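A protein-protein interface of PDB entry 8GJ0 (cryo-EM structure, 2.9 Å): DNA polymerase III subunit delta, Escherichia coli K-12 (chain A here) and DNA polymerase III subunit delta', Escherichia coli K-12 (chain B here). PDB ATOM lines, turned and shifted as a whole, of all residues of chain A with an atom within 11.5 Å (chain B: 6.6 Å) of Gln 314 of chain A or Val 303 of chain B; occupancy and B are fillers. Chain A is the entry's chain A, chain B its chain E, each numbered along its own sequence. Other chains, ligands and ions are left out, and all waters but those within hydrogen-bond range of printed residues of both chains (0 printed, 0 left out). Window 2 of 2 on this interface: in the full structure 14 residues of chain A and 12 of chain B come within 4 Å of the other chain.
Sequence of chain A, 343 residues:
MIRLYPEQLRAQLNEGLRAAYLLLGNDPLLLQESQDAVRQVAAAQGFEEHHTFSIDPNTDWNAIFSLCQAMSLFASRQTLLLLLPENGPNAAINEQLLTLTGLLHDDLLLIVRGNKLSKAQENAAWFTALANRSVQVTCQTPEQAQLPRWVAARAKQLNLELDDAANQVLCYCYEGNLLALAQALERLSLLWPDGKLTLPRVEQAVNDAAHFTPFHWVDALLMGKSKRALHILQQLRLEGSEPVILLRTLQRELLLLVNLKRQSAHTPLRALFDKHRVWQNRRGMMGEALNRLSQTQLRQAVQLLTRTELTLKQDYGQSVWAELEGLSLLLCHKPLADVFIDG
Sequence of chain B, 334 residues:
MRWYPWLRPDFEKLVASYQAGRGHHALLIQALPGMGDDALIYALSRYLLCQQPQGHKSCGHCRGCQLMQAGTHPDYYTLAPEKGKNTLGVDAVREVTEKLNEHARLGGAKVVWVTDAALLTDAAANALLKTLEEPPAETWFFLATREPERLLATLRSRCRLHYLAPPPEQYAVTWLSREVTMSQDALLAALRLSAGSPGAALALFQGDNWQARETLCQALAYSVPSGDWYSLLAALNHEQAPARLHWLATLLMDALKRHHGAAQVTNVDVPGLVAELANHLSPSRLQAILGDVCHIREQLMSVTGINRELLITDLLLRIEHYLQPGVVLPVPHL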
ATOM      1  N   VAL A 244       8.230  24.565 -32.278  1.00  0.00           N
ATOM      2  CA  VAL A 244       7.645  23.226 -32.274  1.00  0.00           C
ATOM      3  C   VAL A 244       7.238  22.825 -33.685  1.00  0.00           C
ATOM      4  O   VAL A 244       7.458  21.684 -34.112  1.00  0.00           O
ATOM      5  CB  VAL A 244       6.449  23.165 -31.306  1.00  0.00           C
ATOM      6  CG1 VAL A 244       5.942  21.735 -31.175  1.00  0.00           C
ATOM      7  CG2 VAL A 244       6.834  23.726 -29.950  1.00  0.00           C
ATOM      8  N   LEU A 247      10.275  21.850 -35.645  1.00  0.00           N
ATOM      9  CA  LEU A 247      10.786  20.540 -35.258  1.00  0.00           C
ATOM     10  C   LEU A 247       9.936  19.422 -35.844  1.00  0.00           C
ATOM     11  O   LEU A 247      10.469  18.438 -36.370  1.00  0.00           O
ATOM     12  CB  LEU A 247      10.838  20.427 -33.734  1.00  0.00           C
ATOM     13  CG  LEU A 247      11.791  21.380 -33.008  1.00  0.00           C
ATOM     14  CD1 LEU A 247      11.601  21.271 -31.506  1.00  0.00           C
ATOM     15  CD2 LEU A 247      13.235  21.098 -33.383  1.00  0.00           C
ATOM     16  N   ARG A 248       8.609  19.553 -35.769  1.00  0.00           N
ATOM     17  CA  ARG A 248       7.749  18.490 -36.279  1.00  0.00           C
ATOM     18  C   ARG A 248       7.817  18.405 -37.798  1.00  0.00           C
ATOM     19  O   ARG A 248       7.736  17.308 -38.365  1.00  0.00           O
ATOM     20  CB  ARG A 248       6.307  18.696 -35.812  1.00  0.00           C
ATOM     21  CG  ARG A 248       6.122  18.737 -34.293  1.00  0.00           C
ATOM     22  CD  ARG A 248       6.818  17.591 -33.569  1.00  0.00           C
ATOM     23  NE  ARG A 248       6.737  17.734 -32.122  1.00  0.00           N
ATOM     24  CZ  ARG A 248       7.507  17.086 -31.259  1.00  0.00           C
ATOM     25  NH1 ARG A 248       8.432  16.229 -31.665  1.00  0.00           N
ATOM     26  NH2 ARG A 248       7.352  17.306 -29.957  1.00  0.00           N
ATOM     27  N   LEU A 305      18.044  16.419 -32.516  1.00  0.00           N
ATOM     28  CA  LEU A 305      16.616  16.708 -32.445  1.00  0.00           C
ATOM     29  C   LEU A 305      16.033  16.268 -31.108  1.00  0.00           C
ATOM     30  O   LEU A 305      15.254  17.003 -30.488  1.00  0.00           O
ATOM     31  CB  LEU A 305      15.890  16.023 -33.602  1.00  0.00           C
ATOM     32  CG  LEU A 305      14.473  16.512 -33.908  1.00  0.00           C
ATOM     33  CD1 LEU A 305      14.501  17.920 -34.479  1.00  0.00           C
ATOM     34  CD2 LEU A 305      13.779  15.561 -34.867  1.00  0.00           C
ATOM     35  N   THR A 306      16.399  15.069 -30.647  1.00  0.00           N
ATOM     36  CA  THR A 306      15.896  14.588 -29.364  1.00  0.00           C
ATOM     37  C   THR A 306      16.364  15.477 -28.219  1.00  0.00           C
ATOM     38  O   THR A 306      15.577  15.822 -27.329  1.00  0.00           O
ATOM     39  CB  THR A 306      16.344  13.146 -29.129  1.00  0.00           C
ATOM     40  OG1 THR A 306      17.746  13.026 -29.401  1.00  0.00           O
ATOM     41  CG2 THR A 306      15.571  12.194 -30.020  1.00  0.00           C
ATOM     42  N   ARG A 307      17.645  15.855 -28.221  1.00  0.00           N
ATOM     43  CA  ARG A 307      18.156  16.714 -27.160  1.00  0.00           C
ATOM     44  C   ARG A 307      17.468  18.073 -27.182  1.00  0.00           C
ATOM     45  O   ARG A 307      17.148  18.631 -26.128  1.00  0.00           O
ATOM     46  CB  ARG A 307      19.673  16.861 -27.294  1.00  0.00           C
ATOM     47  CG  ARG A 307      20.318  17.835 -26.305  1.00  0.00           C
ATOM     48  CD  ARG A 307      20.341  19.267 -26.830  1.00  0.00           C
ATOM     49  NE  ARG A 307      21.655  19.888 -26.705  1.00  0.00           N
ATOM     50  CZ  ARG A 307      22.683  19.627 -27.501  1.00  0.00           C
ATOM     51  NH1 ARG A 307      22.601  18.723 -28.464  1.00  0.00           N
ATOM     52  NH2 ARG A 307      23.822  20.289 -27.326  1.00  0.00           N
ATOM     53  N   THR A 308      17.234  18.622 -28.376  1.00  0.00           N
ATOM     54  CA  THR A 308      16.548  19.904 -28.475  1.00  0.00           C
ATOM     55  C   THR A 308      15.124  19.809 -27.946  1.00  0.00           C
ATOM     56  O   THR A 308      14.661  20.700 -27.227  1.00  0.00           O
ATOM     57  CB  THR A 308      16.548  20.386 -29.926  1.00  0.00           C
ATOM     58  OG1 THR A 308      17.896  20.559 -30.376  1.00  0.00           O
ATOM     59  CG2 THR A 308      15.799  21.703 -30.054  1.00  0.00           C
ATOM     60  N   GLU A 309      14.410  18.735 -28.292  1.00  0.00           N
ATOM     61  CA  GLU A 309      13.051  18.570 -27.788  1.00  0.00           C
ATOM     62  C   GLU A 309      13.041  18.436 -26.270  1.00  0.00           C
ATOM     63  O   GLU A 309      12.190  19.024 -25.590  1.00  0.00           O
ATOM     64  CB  GLU A 309      12.394  17.353 -28.439  1.00  0.00           C
ATOM     65  CG  GLU A 309      10.923  17.188 -28.098  1.00  0.00           C
ATOM     66  CD  GLU A 309      10.286  16.022 -28.825  1.00  0.00           C
ATOM     67  OE1 GLU A 309      11.013  15.291 -29.530  1.00  0.00           O
ATOM     68  OE2 GLU A 309       9.058  15.834 -28.693  1.00  0.00           O
ATOM     69  N   LEU A 310      13.980  17.661 -25.721  1.00  0.00           N
ATOM     70  CA  LEU A 310      14.050  17.510 -24.272  1.00  0.00           C
ATOM     71  C   LEU A 310      14.354  18.840 -23.595  1.00  0.00           C
ATOM     72  O   LEU A 310      13.752  19.174 -22.571  1.00  0.00           O
ATOM     73  CB  LEU A 310      15.104  16.466 -23.902  1.00  0.00           C
ATOM     74  CG  LEU A 310      14.782  15.019 -24.284  1.00  0.00           C
ATOM     75  CD1 LEU A 310      15.974  14.120 -24.000  1.00  0.00           C
ATOM     76  CD2 LEU A 310      13.551  14.520 -23.544  1.00  0.00           C
ATOM     77  N   THR A 311      15.284  19.616 -24.155  1.00  0.00           N
ATOM     78  CA  THR A 311      15.585  20.925 -23.586  1.00  0.00           C
ATOM     79  C   THR A 311      14.367  21.836 -23.646  1.00  0.00           C
ATOM     80  O   THR A 311      14.087  22.576 -22.696  1.00  0.00           O
ATOM     81  CB  THR A 311      16.763  21.560 -24.325  1.00  0.00           C
ATOM     82  OG1 THR A 311      17.912  20.710 -24.221  1.00  0.00           O
ATOM     83  CG2 THR A 311      17.093  22.926 -23.739  1.00  0.00           C
ATOM     84  N   LEU A 312      13.633  21.797 -24.759  1.00  0.00           N
ATOM     85  CA  LEU A 312      12.449  22.638 -24.896  1.00  0.00           C
ATOM     86  C   LEU A 312      11.385  22.275 -23.870  1.00  0.00           C
ATOM     87  O   LEU A 312      10.769  23.160 -23.267  1.00  0.00           O
ATOM     88  CB  LEU A 312      11.889  22.513 -26.314  1.00  0.00           C
ATOM     89  CG  LEU A 312      10.559  23.212 -26.608  1.00  0.00           C
ATOM     90  CD1 LEU A 312      10.701  24.722 -26.527  1.00  0.00           C
ATOM     91  CD2 LEU A 312      10.042  22.796 -27.972  1.00  0.00           C
ATOM     92  N   LYS A 313      11.152  20.979 -23.659  1.00  0.00           N
ATOM     93  CA  LYS A 313      10.011  20.549 -22.855  1.00  0.00           C
ATOM     94  C   LYS A 313      10.365  20.397 -21.376  1.00  0.00           C
ATOM     95  O   LYS A 313       9.763  21.053 -20.521  1.00  0.00           O
ATOM     96  CB  LYS A 313       9.450  19.243 -23.424  1.00  0.00           C
ATOM     97  CG  LYS A 313       8.897  19.407 -24.829  1.00  0.00           C
ATOM     98  CD  LYS A 313       8.156  18.175 -25.305  1.00  0.00           C
ATOM     99  CE  LYS A 313       7.500  18.425 -26.652  1.00  0.00           C
ATOM    100  NZ  LYS A 313       6.666  17.277 -27.089  1.00  0.00           N
ATOM    101  N   GLN A 314      11.330  19.533 -21.058  1.00  0.00           N
ATOM    102  CA  GLN A 314      11.693  19.318 -19.661  1.00  0.00           C
ATOM    103  C   GLN A 314      12.237  20.592 -19.027  1.00  0.00           C
ATOM    104  O   GLN A 314      11.765  21.023 -17.968  1.00  0.00           O
ATOM    105  CB  GLN A 314      12.727  18.196 -19.552  1.00  0.00           C
ATOM    106  CG  GLN A 314      12.152  16.795 -19.626  1.00  0.00           C
ATOM    107  CD  GLN A 314      13.214  15.731 -19.429  1.00  0.00           C
ATOM    108  OE1 GLN A 314      14.387  15.945 -19.740  1.00  0.00           O
ATOM    109  NE2 GLN A 314      12.812  14.581 -18.904  1.00  0.00           N
ATOM    110  N   ASP A 315      13.229  21.213 -19.664  1.00  0.00           N
ATOM    111  CA  ASP A 315      13.933  22.336 -19.063  1.00  0.00           C
ATOM    112  C   ASP A 315      13.301  23.685 -19.372  1.00  0.00           C
ATOM    113  O   ASP A 315      13.597  24.662 -18.675  1.00  0.00           O
ATOM    114  CB  ASP A 315      15.391  22.352 -19.533  1.00  0.00           C
ATOM    115  CG  ASP A 315      16.116  21.058 -19.226  1.00  0.00           C
ATOM    116  OD1 ASP A 315      15.483  20.142 -18.659  1.00  0.00           O
ATOM    117  OD2 ASP A 315      17.318  20.956 -19.550  1.00  0.00           O
ATOM    118  N   TYR A 316      12.440  23.765 -20.386  1.00  0.00           N
ATOM    119  CA  TYR A 316      11.832  25.033 -20.784  1.00  0.00           C
ATOM    120  C   TYR A 316      12.903  26.082 -21.069  1.00  0.00           C
ATOM    121  O   TYR A 316      12.805  27.234 -20.645  1.00  0.00           O
ATOM    122  CB  TYR A 316      10.857  25.528 -19.715  1.00  0.00           C
ATOM    123  CG  TYR A 316       9.808  24.511 -19.328  1.00  0.00           C
ATOM    124  CD1 TYR A 316       8.671  24.330 -20.101  1.00  0.00           C
ATOM    125  CD2 TYR A 316       9.955  23.735 -18.187  1.00  0.00           C
ATOM    126  CE1 TYR A 316       7.711  23.403 -19.751  1.00  0.00           C
ATOM    127  CE2 TYR A 316       9.000  22.805 -17.829  1.00  0.00           C
ATOM    128  CZ  TYR A 316       7.880  22.643 -18.613  1.00  0.00           C
ATOM    129  OH  TYR A 316       6.924  21.718 -18.261  1.00  0.00           O
ATOM    130  N   GLY A 317      13.939  25.675 -21.798  1.00  0.00           N
ATOM    131  CA  GLY A 317      15.043  26.556 -22.108  1.00  0.00           C
ATOM    132  C   GLY A 317      14.703  27.551 -23.200  1.00  0.00           C
ATOM    133  O   GLY A 317      13.598  27.584 -23.742  1.00  0.00           O
ATOM    134  N   GLN A 318      15.694  28.385 -23.523  1.00  0.00           N
ATOM    135  CA  GLN A 318      15.539  29.429 -24.530  1.00  0.00           C
ATOM    136  C   GLN A 318      16.622  29.377 -25.601  1.00  0.00           C
ATOM    137  O   GLN A 318      16.657  30.256 -26.469  1.00  0.00           O
ATOM    138  CB  GLN A 318      15.527  30.817 -23.873  1.00  0.00           C
ATOM    139  CG  GLN A 318      16.794  31.181 -23.101  1.00  0.00           C
ATOM    140  CD  GLN A 318      16.891  30.482 -21.758  1.00  0.00           C
ATOM    141  OE1 GLN A 318      16.030  29.679 -21.400  1.00  0.00           O
ATOM    142  NE2 GLN A 318      17.944  30.784 -21.008  1.00  0.00           N
ATOM    143  N   SER A 319      17.504  28.375 -25.569  1.00  0.00           N
ATOM    144  CA  SER A 319      18.557  28.219 -26.566  1.00  0.00           C
ATOM    145  C   SER A 319      18.140  27.308 -27.713  1.00  0.00           C
ATOM    146  O   SER A 319      18.996  26.669 -28.338  1.00  0.00           O
ATOM    147  CB  SER A 319      19.828  27.688 -25.903  1.00  0.00           C
ATOM    148  OG  SER A 319      19.608  26.408 -25.337  1.00  0.00           O
ATOM    149  N   VAL A 320      16.841  27.232 -28.005  1.00  0.00           N
ATOM    150  CA  VAL A 320      16.364  26.337 -29.055  1.00  0.00           C
ATOM    151  C   VAL A 320      16.884  26.783 -30.415  1.00  0.00           C
ATOM    152  O   VAL A 320      17.255  25.956 -31.255  1.00  0.00           O
ATOM    153  CB  VAL A 320      14.826  26.267 -29.036  1.00  0.00           C
ATOM    154  CG1 VAL A 320      14.321  25.335 -30.127  1.00  0.00           C
ATOM    155  CG2 VAL A 320      14.335  25.813 -27.671  1.00  0.00           C
ATOM    156  N   GLU A 323      20.438  25.690 -31.238  1.00  0.00           N
ATOM    157  CA  GLU A 323      20.477  24.276 -31.590  1.00  0.00           C
ATOM    158  C   GLU A 323      19.906  24.042 -32.983  1.00  0.00           C
ATOM    159  O   GLU A 323      20.397  23.188 -33.727  1.00  0.00           O
ATOM    160  CB  GLU A 323      19.715  23.459 -30.549  1.00  0.00           C
ATOM    161  CG  GLU A 323      20.354  23.482 -29.171  1.00  0.00           C
ATOM    162  CD  GLU A 323      19.523  22.763 -28.128  1.00  0.00           C
ATOM    163  OE1 GLU A 323      18.316  22.558 -28.370  1.00  0.00           O
ATOM    164  OE2 GLU A 323      20.075  22.402 -27.069  1.00  0.00           O
ATOM    165  N   GLU B 298      11.346   5.952 -18.386  1.00  0.00           N
ATOM    166  CA  GLU B 298      11.083   6.991 -17.397  1.00  0.00           C
ATOM    167  C   GLU B 298      10.799   8.328 -18.071  1.00  0.00           C
ATOM    168  O   GLU B 298       9.885   9.055 -17.664  1.00  0.00           O
ATOM    169  CB  GLU B 298      12.267   7.112 -16.437  1.00  0.00           C
ATOM    170  CG  GLU B 298      12.074   8.137 -15.326  1.00  0.00           C
ATOM    171  CD  GLU B 298      10.882   7.826 -14.440  1.00  0.00           C
ATOM    172  OE1 GLU B 298      10.417   6.668 -14.448  1.00  0.00           O
ATOM    173  OE2 GLU B 298      10.409   8.743 -13.736  1.00  0.00           O
ATOM    174  N   GLN B 299      11.572   8.669 -19.104  1.00  0.00           N
ATOM    175  CA  GLN B 299      11.339   9.924 -19.812  1.00  0.00           C
ATOM    176  C   GLN B 299       9.960   9.944 -20.458  1.00  0.00           C
ATOM    177  O   GLN B 299       9.252  10.955 -20.397  1.00  0.00           O
ATOM    178  CB  GLN B 299      12.423  10.145 -20.865  1.00  0.00           C
ATOM    179  CG  GLN B 299      13.762  10.572 -20.296  1.00  0.00           C
ATOM    180  CD  GLN B 299      14.790  10.843 -21.375  1.00  0.00           C
ATOM    181  OE1 GLN B 299      14.767  10.226 -22.438  1.00  0.00           O
ATOM    182  NE2 GLN B 299      15.695  11.777 -21.109  1.00  0.00           N
ATOM    183  N   LEU B 300       9.564   8.836 -21.088  1.00  0.00           N
ATOM    184  CA  LEU B 300       8.249   8.780 -21.717  1.00  0.00           C
ATOM    185  C   LEU B 300       7.138   8.917 -20.685  1.00  0.00           C
ATOM    186  O   LEU B 300       6.146   9.618 -20.919  1.00  0.00           O
ATOM    187  CB  LEU B 300       8.090   7.475 -22.496  1.00  0.00           C
ATOM    188  CG  LEU B 300       8.941   7.313 -23.758  1.00  0.00           C
ATOM    189  CD1 LEU B 300       8.766   5.918 -24.334  1.00  0.00           C
ATOM    190  CD2 LEU B 300       8.586   8.363 -24.796  1.00  0.00           C
ATOM    191  N   MET B 301       7.283   8.256 -19.535  1.00  0.00           N
ATOM    192  CA  MET B 301       6.234   8.310 -18.524  1.00  0.00           C
ATOM    193  C   MET B 301       6.198   9.644 -17.788  1.00  0.00           C
ATOM    194  O   MET B 301       5.146  10.007 -17.248  1.00  0.00           O
ATOM    195  CB  MET B 301       6.414   7.174 -17.518  1.00  0.00           C
ATOM    196  CG  MET B 301       6.191   5.791 -18.107  1.00  0.00           C
ATOM    197  SD  MET B 301       6.276   4.478 -16.875  1.00  0.00           S
ATOM    198  CE  MET B 301       4.830   4.844 -15.882  1.00  0.00           C
ATOM    199  N   SER B 302       7.307  10.381 -17.754  1.00  0.00           N
ATOM    200  CA  SER B 302       7.376  11.623 -16.991  1.00  0.00           C
ATOM    201  C   SER B 302       7.012  12.837 -17.843  1.00  0.00           C
ATOM    202  O   SER B 302       6.090  13.585 -17.506  1.00  0.00           O
ATOM    203  CB  SER B 302       8.779  11.791 -16.396  1.00  0.00           C
ATOM    204  OG  SER B 302       9.760  11.847 -17.416  1.00  0.00           O
ATOM    205  N   VAL B 303       7.731  13.043 -18.949  1.00  0.00           N
ATOM    206  CA  VAL B 303       7.489  14.218 -19.775  1.00  0.00           C
ATOM    207  C   VAL B 303       6.091  14.145 -20.379  1.00  0.00           C
ATOM    208  O   VAL B 303       5.573  13.063 -20.684  1.00  0.00           O
ATOM    209  CB  VAL B 303       8.557  14.346 -20.874  1.00  0.00           C
ATOM    210  CG1 VAL B 303       8.346  15.623 -21.677  1.00  0.00           C
ATOM    211  CG2 VAL B 303       9.951  14.320 -20.269  1.00  0.00           C
ATOM    212  N   THR B 304       5.476  15.312 -20.554  1.00  0.00           N
ATOM    213  CA  THR B 304       4.124  15.421 -21.087  1.00  0.00           C
ATOM    214  C   THR B 304       4.196  15.849 -22.548  1.00  0.00           C
ATOM    215  O   THR B 304       4.810  16.872 -22.870  1.00  0.00           O
ATOM    216  CB  THR B 304       3.300  16.424 -20.280  1.00  0.00           C
ATOM    217  OG1 THR B 304       3.955  17.698 -20.282  1.00  0.00           O
ATOM    218  CG2 THR B 304       3.130  15.945 -18.845  1.00  0.00           C
ATOM    219  N   GLY B 305       3.570  15.067 -23.424  1.00  0.00           N
ATOM    220  CA  GLY B 305       3.553  15.379 -24.836  1.00  0.00           C
ATOM    221  C   GLY B 305       4.820  15.036 -25.585  1.00  0.00           C
ATOM    222  O   GLY B 305       4.956  15.430 -26.749  1.00  0.00           O
ATOM    223  N   ILE B 306       5.756  14.323 -24.956  1.00  0.00           N
ATOM    224  CA  ILE B 306       6.996  13.976 -25.634  1.00  0.00           C
ATOM    225  C   ILE B 306       6.690  13.082 -26.832  1.00  0.00           C
ATOM    226  O   ILE B 306       5.775  12.250 -26.803  1.00  0.00           O
ATOM    227  CB  ILE B 306       7.971  13.289 -24.660  1.00  0.00           C
ATOM    228  CG1 ILE B 306       9.356  13.119 -25.294  1.00  0.00           C
ATOM    229  CG2 ILE B 306       7.429  11.934 -24.225  1.00  0.00           C
ATOM    230  CD1 ILE B 306      10.069  14.423 -25.582  1.00  0.00           C
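The side-chain amino group of Lys 313 of chain A is in hydrogen-bond range of the backbone carbonyl oxygen of Gly 305 of chain B (2.5 Å).
Gln 314 of chain A touches one residue of chain B.
Val 303 of chain B touches one residue of chain A.
Gln 299 of chain B touches just one residue of chain A: Leu 310.
No residue of chain A comes within 4 Å of Ser 302 of chain B.
No residue of chain A comes within 4 Å of Thr 304 of chain B.
Of chain A, only Glu 309 (3.6 Å) and Lys 313 (3.6 Å) come within 4 Å of Ile 306 of chain B.
Printed residues of chain B within 4 Å of Lys 313 of chain A: Gly 305 (2.5 Å) and Ile 306 (3.6 Å).
Printed residues of chain B within 4 Å of Glu 309 of chain A: Ile 306 (3.6 Å).
Of the printed residues of chain B, Leu 310 of chain A touches Gln 299.
Thr 311 of chain A touches none of the printed residues of chain B.
Val 320 of chain A touches none of the printed residues of chain B.
Ile 306 of chain B touches Glu 309 of chain A.
Leu 310 of chain A touches Gln 299 of chain B.
CA of Ile 306 of chain B touches NZ of Lys 313 of chain A (3.6 Å).
Val 303 of chain B touches Gln 314 of chain A.
The guanidinium group (NH2) of Arg 248 of chain A is in salt-bridge range of the side-chain carboxylate (OE2) of Glu 309 of chain A (2.6 Å).
OE2 of Glu 309 of chain A is in salt-bridge range of NZ of Lys 313 of chain A (3.2 Å).
The backbone carbonyl oxygen (O) of Gln 299 of chain B lies within hydrogen-bond range of the side-chain hydroxyl (OG) of Ser 302 of chain B (3.2 Å).
Of the 20 printed residues of chain A, 4 touch a printed residue of chain B.
Hydrophobic or aromatic side chains of chain A within 4 Å of the printed part of chain B: Leu 310.
Printed residues of chain B that touch a printed residue of chain A: Gln 299, Val 303, Gly 305 and Ile 306.
Hydrophobic or aromatic side chains of chain B that line the printed part of chain A: Val 303 and Ile 306.
Among the printed residues, 5 pairs touch across the chains.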
